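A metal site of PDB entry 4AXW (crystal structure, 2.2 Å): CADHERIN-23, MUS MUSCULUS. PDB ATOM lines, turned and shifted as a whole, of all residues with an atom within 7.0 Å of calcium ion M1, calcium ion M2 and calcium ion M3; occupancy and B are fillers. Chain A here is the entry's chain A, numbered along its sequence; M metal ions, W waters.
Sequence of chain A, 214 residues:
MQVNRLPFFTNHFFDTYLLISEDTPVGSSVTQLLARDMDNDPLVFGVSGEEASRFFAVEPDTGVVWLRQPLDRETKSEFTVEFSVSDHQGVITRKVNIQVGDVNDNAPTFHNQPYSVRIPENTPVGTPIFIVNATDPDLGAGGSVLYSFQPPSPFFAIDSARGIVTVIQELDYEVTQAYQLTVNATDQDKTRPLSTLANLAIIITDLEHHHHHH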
ATOM      1  N   GLU A  22     -15.271   3.886   5.860  1.00  0.00           N
ATOM      2  CA  GLU A  22     -15.556   4.921   6.839  1.00  0.00           C
ATOM      3  C   GLU A  22     -14.298   5.514   7.453  1.00  0.00           C
ATOM      4  O   GLU A  22     -14.383   6.545   8.107  1.00  0.00           O
ATOM      5  CB  GLU A  22     -16.508   4.445   7.945  1.00  0.00           C
ATOM      6  CG  GLU A  22     -15.926   3.442   8.925  1.00  0.00           C
ATOM      7  CD  GLU A  22     -16.869   3.111  10.086  1.00  0.00           C
ATOM      8  OE1 GLU A  22     -17.563   4.041  10.539  1.00  0.00           O
ATOM      9  OE2 GLU A  22     -16.863   1.949  10.582  1.00  0.00           O
ATOM     10  N   LEU A  71     -16.919  10.219   7.468  1.00  0.00           N
ATOM     11  CA  LEU A  71     -18.020   9.312   7.299  1.00  0.00           C
ATOM     12  C   LEU A  71     -18.126   8.470   8.593  1.00  0.00           C
ATOM     13  O   LEU A  71     -17.170   8.404   9.342  1.00  0.00           O
ATOM     14  CB  LEU A  71     -17.814   8.417   6.074  1.00  0.00           C
ATOM     15  CG  LEU A  71     -17.816   8.976   4.644  1.00  0.00           C
ATOM     16  CD1 LEU A  71     -17.328   7.907   3.679  1.00  0.00           C
ATOM     17  CD2 LEU A  71     -19.188   9.492   4.169  1.00  0.00           C
ATOM     18  N   ASP A  72     -19.287   7.914   8.884  1.00  0.00           N
ATOM     19  CA  ASP A  72     -19.454   6.995  10.034  1.00  0.00           C
ATOM     20  C   ASP A  72     -20.564   6.025   9.691  1.00  0.00           C
ATOM     21  O   ASP A  72     -21.710   6.398   9.757  1.00  0.00           O
ATOM     22  CB  ASP A  72     -19.815   7.760  11.321  1.00  0.00           C
ATOM     23  CG  ASP A  72     -20.053   6.816  12.539  1.00  0.00           C
ATOM     24  OD1 ASP A  72     -19.742   5.604  12.458  1.00  0.00           O
ATOM     25  OD2 ASP A  72     -20.547   7.285  13.591  1.00  0.00           O
ATOM     26  N   ARG A  73     -20.191   4.789   9.316  1.00  0.00           N
ATOM     27  CA  ARG A  73     -21.114   3.747   8.850  1.00  0.00           C
ATOM     28  C   ARG A  73     -22.210   3.402   9.886  1.00  0.00           C
ATOM     29  O   ARG A  73     -23.323   3.046   9.514  1.00  0.00           O
ATOM     30  CB  ARG A  73     -20.336   2.462   8.554  1.00  0.00           C
ATOM     31  CG  ARG A  73     -21.213   1.377   7.828  1.00  0.00           C
ATOM     32  CD  ARG A  73     -20.772  -0.057   8.066  1.00  0.00           C
ATOM     33  NE  ARG A  73     -20.878  -0.474   9.485  1.00  0.00           N
ATOM     34  CZ  ARG A  73     -21.975  -0.925  10.071  1.00  0.00           C
ATOM     35  NH1 ARG A  73     -23.049  -1.085   9.364  1.00  0.00           N
ATOM     36  NH2 ARG A  73     -22.015  -1.266  11.363  1.00  0.00           N
ATOM     37  N   GLU A  74     -21.869   3.473  11.164  1.00  0.00           N
ATOM     38  CA  GLU A  74     -22.813   3.223  12.230  1.00  0.00           C
ATOM     39  C   GLU A  74     -23.894   4.319  12.327  1.00  0.00           C
ATOM     40  O   GLU A  74     -24.947   4.086  12.946  1.00  0.00           O
ATOM     41  CB  GLU A  74     -22.089   3.109  13.578  1.00  0.00           C
ATOM     42  CG  GLU A  74     -21.313   1.792  13.783  1.00  0.00           C
ATOM     43  CD  GLU A  74     -20.049   1.598  12.897  1.00  0.00           C
ATOM     44  OE1 GLU A  74     -19.189   2.499  12.774  1.00  0.00           O
ATOM     45  OE2 GLU A  74     -19.854   0.491  12.373  1.00  0.00           O
ATOM     46  N   THR A  75     -23.620   5.488  11.745  1.00  0.00           N
ATOM     47  CA  THR A  75     -24.504   6.648  11.838  1.00  0.00           C
ATOM     48  C   THR A  75     -25.277   6.825  10.550  1.00  0.00           C
ATOM     49  O   THR A  75     -26.434   7.156  10.604  1.00  0.00           O
ATOM     50  CB  THR A  75     -23.732   7.965  12.122  1.00  0.00           C
ATOM     51  OG1 THR A  75     -23.424   8.048  13.523  1.00  0.00           O
ATOM     52  CG2 THR A  75     -24.560   9.191  11.714  1.00  0.00           C
ATOM     53  N   GLY A 101     -18.038   1.638   3.742  1.00  0.00           N
ATOM     54  CA  GLY A 101     -17.367   0.452   4.258  1.00  0.00           C
ATOM     55  C   GLY A 101     -17.101   0.515   5.753  1.00  0.00           C
ATOM     56  O   GLY A 101     -16.727   1.549   6.286  1.00  0.00           O
ATOM     57  N   ASP A 102     -17.251  -0.617   6.423  1.00  0.00           N
ATOM     58  CA  ASP A 102     -16.971  -0.720   7.844  1.00  0.00           C
ATOM     59  C   ASP A 102     -15.513  -0.840   8.150  1.00  0.00           C
ATOM     60  O   ASP A 102     -14.773  -1.563   7.434  1.00  0.00           O
ATOM     61  CB  ASP A 102     -17.672  -1.928   8.426  1.00  0.00           C
ATOM     62  CG  ASP A 102     -17.772  -1.856   9.958  1.00  0.00           C
ATOM     63  OD1 ASP A 102     -18.268  -0.810  10.509  1.00  0.00           O
ATOM     64  OD2 ASP A 102     -17.332  -2.844  10.599  1.00  0.00           O
ATOM     65  N   VAL A 103     -15.104  -0.204   9.253  1.00  0.00           N
ATOM     66  CA  VAL A 103     -13.957  -0.654  10.007  1.00  0.00           C
ATOM     67  C   VAL A 103     -14.348  -0.905  11.480  1.00  0.00           C
ATOM     68  O   VAL A 103     -15.386  -0.445  11.965  1.00  0.00           O
ATOM     69  CB  VAL A 103     -12.744   0.336   9.915  1.00  0.00           C
ATOM     70  CG1 VAL A 103     -12.405   0.720   8.426  1.00  0.00           C
ATOM     71  CG2 VAL A 103     -12.948   1.589  10.759  1.00  0.00           C
ATOM     72  N   ASN A 104     -13.524  -1.661  12.196  1.00  0.00           N
ATOM     73  CA  ASN A 104     -13.783  -1.875  13.602  1.00  0.00           C
ATOM     74  C   ASN A 104     -13.413  -0.601  14.362  1.00  0.00           C
ATOM     75  O   ASN A 104     -12.248  -0.359  14.595  1.00  0.00           O
ATOM     76  CB  ASN A 104     -13.025  -3.083  14.129  1.00  0.00           C
ATOM     77  CG  ASN A 104     -13.437  -3.421  15.541  1.00  0.00           C
ATOM     78  OD1 ASN A 104     -14.663  -3.475  15.867  1.00  0.00           O
ATOM     79  ND2 ASN A 104     -12.432  -3.608  16.419  1.00  0.00           N
ATOM     80  N   ASP A 105     -14.379   0.254  14.672  1.00  0.00           N
ATOM     81  CA  ASP A 105     -14.067   1.460  15.454  1.00  0.00           C
ATOM     82  C   ASP A 105     -14.925   1.603  16.676  1.00  0.00           C
ATOM     83  O   ASP A 105     -14.930   2.676  17.276  1.00  0.00           O
ATOM     84  CB  ASP A 105     -14.141   2.742  14.617  1.00  0.00           C
ATOM     85  CG  ASP A 105     -15.460   2.877  13.765  1.00  0.00           C
ATOM     86  OD1 ASP A 105     -16.345   1.964  13.719  1.00  0.00           O
ATOM     87  OD2 ASP A 105     -15.552   3.911  13.058  1.00  0.00           O
ATOM     88  N   ASN A 106     -15.641   0.561  17.074  1.00  0.00           N
ATOM     89  CA  ASN A 106     -16.333   0.595  18.353  1.00  0.00           C
ATOM     90  C   ASN A 106     -15.898  -0.477  19.277  1.00  0.00           C
ATOM     91  O   ASN A 106     -15.645  -1.608  18.847  1.00  0.00           O
ATOM     92  CB  ASN A 106     -17.829   0.494  18.138  1.00  0.00           C
ATOM     93  CG  ASN A 106     -18.390   1.677  17.397  1.00  0.00           C
ATOM     94  OD1 ASN A 106     -18.970   2.541  18.005  1.00  0.00           O
ATOM     95  ND2 ASN A 106     -18.156   1.745  16.070  1.00  0.00           N
ATOM     96  N   ALA A 107     -15.864  -0.153  20.561  1.00  0.00           N
ATOM     97  CA  ALA A 107     -15.707  -1.195  21.586  1.00  0.00           C
ATOM     98  C   ALA A 107     -17.086  -1.681  22.038  1.00  0.00           C
ATOM     99  O   ALA A 107     -18.071  -0.966  21.867  1.00  0.00           O
ATOM    100  CB  ALA A 107     -14.927  -0.610  22.760  1.00  0.00           C
ATOM    101  N   PRO A 108     -17.166  -2.874  22.653  1.00  0.00           N
ATOM    102  CA  PRO A 108     -18.465  -3.310  23.241  1.00  0.00           C
ATOM    103  C   PRO A 108     -19.014  -2.434  24.366  1.00  0.00           C
ATOM    104  O   PRO A 108     -18.243  -1.778  25.047  1.00  0.00           O
ATOM    105  CB  PRO A 108     -18.200  -4.718  23.766  1.00  0.00           C
ATOM    106  CG  PRO A 108     -16.935  -5.159  23.106  1.00  0.00           C
ATOM    107  CD  PRO A 108     -16.136  -3.932  22.757  1.00  0.00           C
ATOM    108  N   ASP A 136     -21.972  -4.763  20.362  1.00  0.00           N
ATOM    109  CA  ASP A 136     -20.928  -4.049  19.614  1.00  0.00           C
ATOM    110  C   ASP A 136     -21.476  -3.860  18.208  1.00  0.00           C
ATOM    111  O   ASP A 136     -21.777  -4.831  17.551  1.00  0.00           O
ATOM    112  CB  ASP A 136     -19.621  -4.869  19.599  1.00  0.00           C
ATOM    113  CG  ASP A 136     -18.451  -4.117  18.986  1.00  0.00           C
ATOM    114  OD1 ASP A 136     -18.650  -3.468  17.913  1.00  0.00           O
ATOM    115  OD2 ASP A 136     -17.309  -4.250  19.509  1.00  0.00           O
ATOM    116  N   PRO A 137     -21.613  -2.621  17.732  1.00  0.00           N
ATOM    117  CA  PRO A 137     -22.322  -2.394  16.458  1.00  0.00           C
ATOM    118  C   PRO A 137     -21.470  -2.515  15.166  1.00  0.00           C
ATOM    119  O   PRO A 137     -22.015  -2.346  14.077  1.00  0.00           O
ATOM    120  CB  PRO A 137     -22.807  -0.949  16.595  1.00  0.00           C
ATOM    121  CG  PRO A 137     -21.623  -0.297  17.289  1.00  0.00           C
ATOM    122  CD  PRO A 137     -21.086  -1.382  18.280  1.00  0.00           C
ATOM    123  N   ASP A 138     -20.179  -2.782  15.265  1.00  0.00           N
ATOM    124  CA  ASP A 138     -19.371  -3.033  14.080  1.00  0.00           C
ATOM    125  C   ASP A 138     -19.787  -4.318  13.371  1.00  0.00           C
ATOM    126  O   ASP A 138     -20.486  -5.128  13.949  1.00  0.00           O
ATOM    127  CB  ASP A 138     -17.905  -3.099  14.440  1.00  0.00           C
ATOM    128  CG  ASP A 138     -17.383  -1.791  15.053  1.00  0.00           C
ATOM    129  OD1 ASP A 138     -17.424  -0.753  14.335  1.00  0.00           O
ATOM    130  OD2 ASP A 138     -16.918  -1.822  16.222  1.00  0.00           O
ATOM    131  N   LEU A 139     -19.375  -4.502  12.121  1.00  0.00           N
ATOM    132  CA  LEU A 139     -19.747  -5.700  11.369  1.00  0.00           C
ATOM    133  C   LEU A 139     -18.800  -6.841  11.652  1.00  0.00           C
ATOM    134  O   LEU A 139     -17.590  -6.611  11.837  1.00  0.00           O
ATOM    135  CB  LEU A 139     -19.686  -5.426   9.854  1.00  0.00           C
ATOM    136  CG  LEU A 139     -20.680  -4.414   9.306  1.00  0.00           C
ATOM    137  CD1 LEU A 139     -20.565  -4.434   7.811  1.00  0.00           C
ATOM    138  CD2 LEU A 139     -22.156  -4.683   9.761  1.00  0.00           C
ATOM    139  N   ALA A 141     -16.544 -10.103  12.606  1.00  0.00           N
ATOM    140  CA  ALA A 141     -15.712 -10.343  13.796  1.00  0.00           C
ATOM    141  C   ALA A 141     -15.608  -9.121  14.712  1.00  0.00           C
ATOM    142  O   ALA A 141     -15.597  -9.225  15.937  1.00  0.00           O
ATOM    143  CB  ALA A 141     -14.346 -10.822  13.390  1.00  0.00           C
ATOM    144  N   GLY A 142     -15.617  -7.936  14.122  1.00  0.00           N
ATOM    145  CA  GLY A 142     -15.599  -6.714  14.936  1.00  0.00           C
ATOM    146  C   GLY A 142     -16.837  -6.454  15.768  1.00  0.00           C
ATOM    147  O   GLY A 142     -16.831  -5.549  16.575  1.00  0.00           O
ATOM    148  N   GLY A 143     -17.876  -7.245  15.572  1.00  0.00           N
ATOM    149  CA  GLY A 143     -19.128  -7.093  16.342  1.00  0.00           C
ATOM    150  C   GLY A 143     -19.470  -8.321  17.176  1.00  0.00           C
ATOM    151  O   GLY A 143     -20.500  -8.375  17.787  1.00  0.00           O
ATOM    152  N   SER A 144     -18.595  -9.310  17.214  1.00  0.00           N
ATOM    153  CA  SER A 144     -18.879 -10.550  17.935  1.00  0.00           C
ATOM    154  C   SER A 144     -18.093 -10.485  19.222  1.00  0.00           C
ATOM    155  O   SER A 144     -16.889 -10.379  19.173  1.00  0.00           O
ATOM    156  CB  SER A 144     -18.415 -11.736  17.084  1.00  0.00           C
ATOM    157  OG  SER A 144     -18.654 -12.970  17.742  1.00  0.00           O
ATOM    158  N   THR A 186     -14.521  -8.167  24.688  1.00  0.00           N
ATOM    159  CA  THR A 186     -13.721  -7.767  23.536  1.00  0.00           C
ATOM    160  C   THR A 186     -14.440  -8.202  22.268  1.00  0.00           C
ATOM    161  O   THR A 186     -15.147  -9.252  22.250  1.00  0.00           O
ATOM    162  CB  THR A 186     -12.321  -8.408  23.564  1.00  0.00           C
ATOM    163  OG1 THR A 186     -11.567  -8.033  22.376  1.00  0.00           O
ATOM    164  CG2 THR A 186     -12.404  -9.938  23.669  1.00  0.00           C
ATOM    165  N   ASP A 187     -14.298  -7.406  21.220  1.00  0.00           N
ATOM    166  CA  ASP A 187     -14.615  -7.895  19.902  1.00  0.00           C
ATOM    167  C   ASP A 187     -13.436  -8.727  19.379  1.00  0.00           C
ATOM    168  O   ASP A 187     -12.419  -8.876  20.091  1.00  0.00           O
ATOM    169  CB  ASP A 187     -15.051  -6.799  18.930  1.00  0.00           C
ATOM    170  CG  ASP A 187     -13.980  -5.795  18.638  1.00  0.00           C
ATOM    171  OD1 ASP A 187     -12.806  -6.210  18.507  1.00  0.00           O
ATOM    172  OD2 ASP A 187     -14.341  -4.580  18.486  1.00  0.00           O
ATOM    173  N   GLN A 188     -13.616  -9.316  18.181  1.00  0.00           N
ATOM    174  CA  GLN A 188     -12.677 -10.306  17.630  1.00  0.00           C
ATOM    175  C   GLN A 188     -12.049  -9.857  16.331  1.00  0.00           C
ATOM    176  O   GLN A 188     -11.601 -10.665  15.535  1.00  0.00           O
ATOM    177  CB  GLN A 188     -13.401 -11.607  17.379  1.00  0.00           C
ATOM    178  CG  GLN A 188     -13.856 -12.309  18.663  1.00  0.00           C
ATOM    179  CD  GLN A 188     -14.460 -13.682  18.399  1.00  0.00           C
ATOM    180  OE1 GLN A 188     -13.731 -14.692  18.330  1.00  0.00           O
ATOM    181  NE2 GLN A 188     -15.787 -13.725  18.225  1.00  0.00           N
ATOM    182  N   ASP A 189     -12.036  -8.558  16.092  1.00  0.00           N
ATOM    183  CA  ASP A 189     -11.379  -8.018  14.921  1.00  0.00           C
ATOM    184  C   ASP A 189      -9.936  -8.497  14.914  1.00  0.00           C
ATOM    185  O   ASP A 189      -9.243  -8.396  15.930  1.00  0.00           O
ATOM    186  CB  ASP A 189     -11.362  -6.517  14.962  1.00  0.00           C
ATOM    187  CG  ASP A 189     -10.890  -5.912  13.655  1.00  0.00           C
ATOM    188  OD1 ASP A 189     -11.630  -5.982  12.625  1.00  0.00           O
ATOM    189  OD2 ASP A 189      -9.808  -5.300  13.678  1.00  0.00           O
ATOM    190  N   ARG A 192      -7.193  -4.940  14.830  1.00  0.00           N
ATOM    191  CA  ARG A 192      -7.434  -3.966  15.881  1.00  0.00           C
ATOM    192  C   ARG A 192      -8.594  -4.362  16.832  1.00  0.00           C
ATOM    193  O   ARG A 192      -9.594  -3.668  16.952  1.00  0.00           O
ATOM    194  CB  ARG A 192      -7.686  -2.591  15.220  1.00  0.00           C
ATOM    195  CG  ARG A 192      -6.542  -2.116  14.308  1.00  0.00           C
ATOM    196  CD  ARG A 192      -6.772  -0.770  13.648  1.00  0.00           C
ATOM    197  NE  ARG A 192      -7.001   0.241  14.673  1.00  0.00           N
ATOM    198  CZ  ARG A 192      -8.188   0.726  15.025  1.00  0.00           C
ATOM    199  NH1 ARG A 192      -9.294   0.380  14.361  1.00  0.00           N
ATOM    200  NH2 ARG A 192      -8.260   1.555  16.070  1.00  0.00           N
ATOM    201  N   PRO A 193      -8.462  -5.457  17.567  1.00  0.00           N
ATOM    202  CA  PRO A 193      -9.532  -5.703  18.551  1.00  0.00           C
ATOM    203  C   PRO A 193      -9.793  -4.566  19.583  1.00  0.00           C
ATOM    204  O   PRO A 193      -8.857  -3.937  20.086  1.00  0.00           O
ATOM    205  CB  PRO A 193      -9.057  -6.940  19.273  1.00  0.00           C
ATOM    206  CG  PRO A 193      -7.525  -6.904  19.131  1.00  0.00           C
ATOM    207  CD  PRO A 193      -7.283  -6.327  17.763  1.00  0.00           C
ATOM    208  N   LEU A 194     -11.050  -4.347  19.940  1.00  0.00           N
ATOM    209  CA  LEU A 194     -11.347  -3.335  20.960  1.00  0.00           C
ATOM    210  C   LEU A 194     -12.121  -3.949  22.095  1.00  0.00           C
ATOM    211  O   LEU A 194     -12.925  -4.908  21.901  1.00  0.00           O
ATOM    212  CB  LEU A 194     -12.149  -2.166  20.356  1.00  0.00           C
ATOM    213  CG  LEU A 194     -11.459  -1.369  19.227  1.00  0.00           C
ATOM    214  CD1 LEU A 194     -12.471  -0.451  18.544  1.00  0.00           C
ATOM    215  CD2 LEU A 194     -10.261  -0.531  19.781  1.00  0.00           C
HETATM  216 CA    CA M   1     -17.447   0.513  12.268  1.00  0.00          CA
HETATM  217 CA    CA M   2     -17.912   4.381  12.828  1.00  0.00          CA
HETATM  218 CA    CA M   3     -16.166  -3.489  17.651  1.00  0.00          CA
HETATM  219  O   HOH W   1     -18.332   4.739  15.052  1.00  0.00           O
HETATM  220  O   HOH W   2     -16.923   6.594  12.829  1.00  0.00           O
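The side-chain carboxylate of Asp 72 sits at hydrogen-bond distance from the side-chain hydroxyl of Thr 75 (3.0 Å). The side-chain carboxylate of Asp 187 is in hydrogen-bond range of the backbone NH of Asp 189 (3.5 Å). ND2 of Asn 106 sits close to OD1 of Asp 105 (3.0 Å). The backbone NH (N) of Arg 73 sits close to the side-chain carboxylate (OE1) of Glu 22. The backbone NH (N) of Glu 22 lies within hydrogen-bond range of the backbone carbonyl oxygen (O) of Gly 101 (2.8 Å). The backbone carbonyl oxygen (O) of Arg 192 is in hydrogen-bond range of the side-chain amide nitrogen (ND2) of Asn 104, 2.9 Å away. The side-chain carboxylate (OD1) of Asp 102 sits close to the guanidinium group (NE) of Arg 73, at 2.8 Å. The backbone NH (N) of Leu 139 sits at hydrogen-bond distance from the side-chain carboxylate (OD2) of Asp 102, at 3.0 Å.
Six residues have an atom within 4 Å of calcium ion M1: Glu 22, Glu 74, Asp 102, Val 103, Asp 105 and Asp 138.
Within 4 Å of calcium ion M2: Glu 22, Asp 72, Glu 74 and Asp 105. The nearest printed residue that does not touch calcium ion M2 is Asn 106 (4.2 Å).
Calcium ion M1 is bound by the side-chain carboxylate (OE2) of Glu 22 (2.3 Å), the backbone carbonyl oxygen (O) of Val 103 (2.3 Å), the side-chain carboxylate (OD1) of Asp 105 (2.3 Å), the side-chain carboxylate (OD1) of Asp 102 (2.3 Å), the side-chain carboxylate (OE2) of Glu 74 (2.4 Å), the side-chain carboxylate (OD1) of Asp 138 (2.4 Å) and the side-chain carboxylate (OE1) of Glu 74 (2.7 Å). Calcium ion M1 has seven donor atoms within binding distance.
Calcium ion M2 is bound by the side-chain carboxylate (OD1) of Asp 72, the side-chain carboxylate (OE1) of Glu 74, water W1, the side-chain carboxylate (OE1) of Glu 22, the side-chain carboxylate (OD2) of Asp 105 and water W2. Slightly farther from calcium ion M2 lies the side-chain carboxylate (OD1) of Asp 105 (3.0 Å).
OD2 of Asp 187 is bound to calcium ion M3 (2.3 Å). Calcium ion M3 is bound by the backbone carbonyl oxygen (O) of Asn 106. OD2 of Asp 136 is bound to calcium ion M3 (2.3 Å). Calcium ion M3 is bound by OD2 of Asp 138, 2.3 Å away. OD1 of Asn 104 binds calcium ion M3. Calcium ion M3 is bound by O of Gly 142. OD1 of Asp 136 binds calcium ion M3 (2.5 Å). Calcium ion M3 has seven donor atoms within binding distance.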
